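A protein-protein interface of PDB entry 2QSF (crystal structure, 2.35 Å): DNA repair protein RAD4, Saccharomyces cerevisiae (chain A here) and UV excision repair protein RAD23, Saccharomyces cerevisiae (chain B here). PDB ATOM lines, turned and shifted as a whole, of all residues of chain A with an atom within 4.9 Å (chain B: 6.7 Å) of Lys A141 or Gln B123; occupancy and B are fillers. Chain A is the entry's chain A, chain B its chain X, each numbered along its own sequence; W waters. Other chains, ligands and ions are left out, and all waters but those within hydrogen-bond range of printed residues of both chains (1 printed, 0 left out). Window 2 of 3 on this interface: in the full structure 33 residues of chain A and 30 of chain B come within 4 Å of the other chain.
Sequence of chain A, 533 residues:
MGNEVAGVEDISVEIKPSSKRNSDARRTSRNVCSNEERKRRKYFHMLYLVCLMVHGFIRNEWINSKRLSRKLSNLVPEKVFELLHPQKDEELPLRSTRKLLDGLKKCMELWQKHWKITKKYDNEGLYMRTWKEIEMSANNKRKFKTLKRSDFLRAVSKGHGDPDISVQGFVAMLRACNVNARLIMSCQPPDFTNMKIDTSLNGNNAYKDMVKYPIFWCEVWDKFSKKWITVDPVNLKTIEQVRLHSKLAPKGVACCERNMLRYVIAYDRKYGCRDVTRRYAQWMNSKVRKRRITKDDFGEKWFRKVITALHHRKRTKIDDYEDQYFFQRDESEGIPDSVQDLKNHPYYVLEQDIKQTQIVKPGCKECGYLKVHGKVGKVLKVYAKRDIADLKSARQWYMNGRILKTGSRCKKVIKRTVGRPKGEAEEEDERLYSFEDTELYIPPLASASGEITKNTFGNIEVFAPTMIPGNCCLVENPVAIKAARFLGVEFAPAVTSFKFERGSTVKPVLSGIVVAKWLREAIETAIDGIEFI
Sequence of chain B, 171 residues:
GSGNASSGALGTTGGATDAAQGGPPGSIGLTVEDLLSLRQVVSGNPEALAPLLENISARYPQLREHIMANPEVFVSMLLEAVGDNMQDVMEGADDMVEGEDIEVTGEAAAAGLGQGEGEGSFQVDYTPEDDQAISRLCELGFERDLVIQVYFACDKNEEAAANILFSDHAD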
ATOM      1  N   SER A 137       1.042  26.625  -3.161  1.00  0.00           N
ATOM      2  CA  SER A 137       0.974  25.701  -2.035  1.00  0.00           C
ATOM      3  C   SER A 137       1.630  24.352  -2.329  1.00  0.00           C
ATOM      4  O   SER A 137       1.865  23.561  -1.418  1.00  0.00           O
ATOM      5  CB  SER A 137      -0.477  25.506  -1.585  1.00  0.00           C
ATOM      6  OG  SER A 137      -1.268  24.949  -2.617  1.00  0.00           O
ATOM      7  N   ALA A 138       1.941  24.087  -3.595  1.00  0.00           N
ATOM      8  CA  ALA A 138       2.599  22.832  -3.958  1.00  0.00           C
ATOM      9  C   ALA A 138       4.125  23.000  -3.895  1.00  0.00           C
ATOM     10  O   ALA A 138       4.838  22.095  -3.461  1.00  0.00           O
ATOM     11  CB  ALA A 138       2.175  22.401  -5.350  1.00  0.00           C
ATOM     12  N   ASN A 139       4.616  24.164  -4.314  1.00  0.00           N
ATOM     13  CA  ASN A 139       6.051  24.451  -4.302  1.00  0.00           C
ATOM     14  C   ASN A 139       6.542  24.857  -2.922  1.00  0.00           C
ATOM     15  O   ASN A 139       7.705  24.662  -2.586  1.00  0.00           O
ATOM     16  CB  ASN A 139       6.381  25.574  -5.284  1.00  0.00           C
ATOM     17  CG  ASN A 139       6.001  25.231  -6.702  1.00  0.00           C
ATOM     18  OD1 ASN A 139       4.821  25.063  -7.016  1.00  0.00           O
ATOM     19  ND2 ASN A 139       7.001  25.122  -7.573  1.00  0.00           N
ATOM     20  N   ASN A 140       5.655  25.456  -2.137  1.00  0.00           N
ATOM     21  CA  ASN A 140       5.983  25.883  -0.786  1.00  0.00           C
ATOM     22  C   ASN A 140       5.292  24.915   0.171  1.00  0.00           C
ATOM     23  O   ASN A 140       4.476  25.318   1.000  1.00  0.00           O
ATOM     24  CB  ASN A 140       5.489  27.316  -0.548  1.00  0.00           C
ATOM     25  CG  ASN A 140       6.280  28.346  -1.341  1.00  0.00           C
ATOM     26  OD1 ASN A 140       6.402  28.252  -2.563  1.00  0.00           O
ATOM     27  ND2 ASN A 140       6.818  29.340  -0.645  1.00  0.00           N
ATOM     28  N   LYS A 141       5.626  23.632   0.037  1.00  0.00           N
ATOM     29  CA  LYS A 141       5.035  22.594   0.868  1.00  0.00           C
ATOM     30  C   LYS A 141       5.017  22.886   2.354  1.00  0.00           C
ATOM     31  O   LYS A 141       5.982  23.394   2.915  1.00  0.00           O
ATOM     32  CB  LYS A 141       5.736  21.251   0.650  1.00  0.00           C
ATOM     33  CG  LYS A 141       5.005  20.325  -0.310  1.00  0.00           C
ATOM     34  CD  LYS A 141       5.189  18.859   0.070  1.00  0.00           C
ATOM     35  CE  LYS A 141       6.660  18.462   0.098  1.00  0.00           C
ATOM     36  NZ  LYS A 141       7.370  18.715  -1.195  1.00  0.00           N
ATOM     37  N   ARG A 142       3.889  22.563   2.978  1.00  0.00           N
ATOM     38  CA  ARG A 142       3.712  22.731   4.405  1.00  0.00           C
ATOM     39  C   ARG A 142       3.478  21.348   4.992  1.00  0.00           C
ATOM     40  O   ARG A 142       3.137  20.406   4.287  1.00  0.00           O
ATOM     41  CB  ARG A 142       2.523  23.635   4.712  1.00  0.00           C
ATOM     42  CG  ARG A 142       2.711  25.050   4.220  1.00  0.00           C
ATOM     43  CD  ARG A 142       1.603  25.968   4.691  1.00  0.00           C
ATOM     44  NE  ARG A 142       1.843  27.342   4.259  1.00  0.00           N
ATOM     45  CZ  ARG A 142       0.939  28.314   4.311  1.00  0.00           C
ATOM     46  NH1 ARG A 142      -0.278  28.071   4.780  1.00  0.00           N
ATOM     47  NH2 ARG A 142       1.246  29.532   3.882  1.00  0.00           N
ATOM     48  N   LYS A 143       3.696  21.243   6.291  1.00  0.00           N
ATOM     49  CA  LYS A 143       3.527  20.007   7.031  1.00  0.00           C
ATOM     50  C   LYS A 143       2.325  20.344   7.913  1.00  0.00           C
ATOM     51  O   LYS A 143       2.210  21.472   8.380  1.00  0.00           O
ATOM     52  CB  LYS A 143       4.773  19.781   7.889  1.00  0.00           C
ATOM     53  CG  LYS A 143       5.291  18.369   8.006  1.00  0.00           C
ATOM     54  CD  LYS A 143       6.568  18.388   8.851  1.00  0.00           C
ATOM     55  CE  LYS A 143       7.198  17.010   9.003  1.00  0.00           C
ATOM     56  NZ  LYS A 143       7.861  16.547   7.750  1.00  0.00           N
ATOM     57  N   PHE A 144       1.430  19.390   8.132  1.00  0.00           N
ATOM     58  CA  PHE A 144       0.268  19.652   8.957  1.00  0.00           C
ATOM     59  C   PHE A 144       0.206  18.678  10.123  1.00  0.00           C
ATOM     60  O   PHE A 144       0.487  17.491   9.975  1.00  0.00           O
ATOM     61  CB  PHE A 144      -1.010  19.543   8.113  1.00  0.00           C
ATOM     62  CG  PHE A 144      -1.047  20.491   6.944  1.00  0.00           C
ATOM     63  CD1 PHE A 144      -1.468  21.801   7.104  1.00  0.00           C
ATOM     64  CD2 PHE A 144      -0.613  20.074   5.686  1.00  0.00           C
ATOM     65  CE1 PHE A 144      -1.455  22.680   6.043  1.00  0.00           C
ATOM     66  CE2 PHE A 144      -0.597  20.949   4.613  1.00  0.00           C
ATOM     67  CZ  PHE A 144      -1.017  22.257   4.791  1.00  0.00           C
ATOM     68  N   SER B 121       1.958  13.826  11.854  1.00  0.00           N
ATOM     69  CA  SER B 121       1.889  14.919  10.897  1.00  0.00           C
ATOM     70  C   SER B 121       1.667  14.355   9.496  1.00  0.00           C
ATOM     71  O   SER B 121       1.809  13.157   9.277  1.00  0.00           O
ATOM     72  CB  SER B 121       3.212  15.695  10.942  1.00  0.00           C
ATOM     73  OG  SER B 121       3.182  16.844  10.114  1.00  0.00           O
ATOM     74  N   PHE B 122       1.289  15.211   8.553  1.00  0.00           N
ATOM     75  CA  PHE B 122       1.103  14.768   7.178  1.00  0.00           C
ATOM     76  C   PHE B 122       1.386  15.911   6.211  1.00  0.00           C
ATOM     77  O   PHE B 122       1.539  17.056   6.621  1.00  0.00           O
ATOM     78  CB  PHE B 122      -0.306  14.185   6.955  1.00  0.00           C
ATOM     79  CG  PHE B 122      -1.409  15.206   6.904  1.00  0.00           C
ATOM     80  CD1 PHE B 122      -2.068  15.603   8.065  1.00  0.00           C
ATOM     81  CD2 PHE B 122      -1.803  15.758   5.685  1.00  0.00           C
ATOM     82  CE1 PHE B 122      -3.102  16.530   8.011  1.00  0.00           C
ATOM     83  CE2 PHE B 122      -2.830  16.684   5.619  1.00  0.00           C
ATOM     84  CZ  PHE B 122      -3.483  17.072   6.785  1.00  0.00           C
ATOM     85  N   GLN B 123       1.499  15.586   4.932  1.00  0.00           N
ATOM     86  CA  GLN B 123       1.772  16.573   3.902  1.00  0.00           C
ATOM     87  C   GLN B 123       1.200  16.023   2.608  1.00  0.00           C
ATOM     88  O   GLN B 123       0.944  14.824   2.502  1.00  0.00           O
ATOM     89  CB  GLN B 123       3.284  16.808   3.766  1.00  0.00           C
ATOM     90  CG  GLN B 123       4.123  15.543   3.890  1.00  0.00           C
ATOM     91  CD  GLN B 123       5.628  15.794   3.798  1.00  0.00           C
ATOM     92  OE1 GLN B 123       6.197  15.892   2.703  1.00  0.00           O
ATOM     93  NE2 GLN B 123       6.277  15.897   4.951  1.00  0.00           N
ATOM     94  N   VAL B 124       0.964  16.892   1.633  1.00  0.00           N
ATOM     95  CA  VAL B 124       0.430  16.422   0.368  1.00  0.00           C
ATOM     96  C   VAL B 124       1.573  16.411  -0.648  1.00  0.00           C
ATOM     97  O   VAL B 124       2.133  17.450  -1.006  1.00  0.00           O
ATOM     98  CB  VAL B 124      -0.803  17.290  -0.096  1.00  0.00           C
ATOM     99  CG1 VAL B 124      -1.577  17.796   1.143  1.00  0.00           C
ATOM    100  CG2 VAL B 124      -0.390  18.419  -0.977  1.00  0.00           C
ATOM    101  N   ASP B 125       1.946  15.206  -1.067  1.00  0.00           N
ATOM    102  CA  ASP B 125       3.032  15.019  -2.023  1.00  0.00           C
ATOM    103  C   ASP B 125       2.541  14.308  -3.265  1.00  0.00           C
ATOM    104  O   ASP B 125       1.464  13.717  -3.275  1.00  0.00           O
ATOM    105  CB  ASP B 125       4.153  14.136  -1.449  1.00  0.00           C
ATOM    106  CG  ASP B 125       4.860  14.747  -0.258  1.00  0.00           C
ATOM    107  OD1 ASP B 125       5.188  15.955  -0.289  1.00  0.00           O
ATOM    108  OD2 ASP B 125       5.112  13.993   0.708  1.00  0.00           O
ATOM    109  N   TYR B 126       3.356  14.373  -4.308  1.00  0.00           N
ATOM    110  CA  TYR B 126       3.087  13.673  -5.549  1.00  0.00           C
ATOM    111  C   TYR B 126       3.997  12.458  -5.398  1.00  0.00           C
ATOM    112  O   TYR B 126       4.969  12.504  -4.636  1.00  0.00           O
ATOM    113  CB  TYR B 126       3.523  14.504  -6.763  1.00  0.00           C
ATOM    114  CG  TYR B 126       2.509  15.529  -7.214  1.00  0.00           C
ATOM    115  CD1 TYR B 126       2.872  16.860  -7.403  1.00  0.00           C
ATOM    116  CD2 TYR B 126       1.181  15.170  -7.439  1.00  0.00           C
ATOM    117  CE1 TYR B 126       1.934  17.818  -7.804  1.00  0.00           C
ATOM    118  CE2 TYR B 126       0.233  16.116  -7.843  1.00  0.00           C
ATOM    119  CZ  TYR B 126       0.617  17.437  -8.022  1.00  0.00           C
ATOM    120  OH  TYR B 126      -0.318  18.370  -8.422  1.00  0.00           O
ATOM    121  N   ASP B 131       6.698  12.982  -9.510  1.00  0.00           N
ATOM    122  CA  ASP B 131       7.491  14.192  -9.279  1.00  0.00           C
ATOM    123  C   ASP B 131       8.628  14.285 -10.301  1.00  0.00           C
ATOM    124  O   ASP B 131       8.840  15.316 -10.946  1.00  0.00           O
ATOM    125  CB  ASP B 131       8.116  14.179  -7.874  1.00  0.00           C
ATOM    126  CG  ASP B 131       7.330  15.001  -6.858  1.00  0.00           C
ATOM    127  OD1 ASP B 131       6.844  16.094  -7.223  1.00  0.00           O
ATOM    128  OD2 ASP B 131       7.224  14.560  -5.685  1.00  0.00           O
HETATM  129  O   HOH W   1       1.377  19.772   1.985  1.00  0.00           O
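Among the printed residues, pairs that only touch across the chains: Lys A141 with Gln B123, Lys A141 with Val B124, Arg A142 with Gln B123, Lys A143 with Ser B121 and Lys A143 with Phe B122.
The side-chain amide oxygen of Gln B123 lies close to the side-chain carboxylate of Asp B125 (3.0 Å).
Water W1 bridges the backbone NH (N) of Val B124 (2.9 Å) and the backbone carbonyl oxygen (O) of Arg A142 (3.0 Å).
Hydrophobic or aromatic side chains of chain A within 4 Å of the printed part of chain B: Phe A144.
Along chain A the printed residues that touch a printed residue of chain B span positions 141 to 144.
Among the printed residues, 9 pairs touch across the chains.
Among the printed residues, Asp or Glu carboxylates within 4 Å of a Lys or Arg side-chain nitrogen of the other chain: Lys A141 with Asp B125.
The side-chain carboxylate (OD1) of Asp B125 lies within salt-bridge range of the side-chain amino group (NZ) of Lys A141.
NE2 of Gln B123 lies close to NZ of Lys A143.
The side-chain hydroxyl (OG) of Ser B121 sits at hydrogen-bond distance from the backbone carbonyl oxygen (O) of Phe A144, at 2.8 Å.
The backbone carbonyl oxygen of Phe B122 lies within hydrogen-bond range of the backbone NH of Phe A144 (2.8 Å).
Of the printed residues of chain B, Arg A142 touches Gln B123 (3.6 Å).
Of the printed residues of chain B, Phe A144 touches Ser B121 and Phe B122.
Printed residues of chain A within 4 Å of Phe B122: Lys A143 (3.6 Å) and Phe A144 (2.8 Å).
Gln B123 touches just these residues of chain A: Lys A141 (3.7 Å), Arg A142 (3.6 Å) and Lys A143 (3.3 Å).
Of the printed residues of chain A, Val B124 touches Lys A141 (3.5 Å).
Of the printed residues of chain A, Asp B125 touches Lys A141.
Tyr B126 touches none of the printed residues of chain A.
The nearest residue of chain B that does not touch Lys A141 is Asp B131 (6.1 Å).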
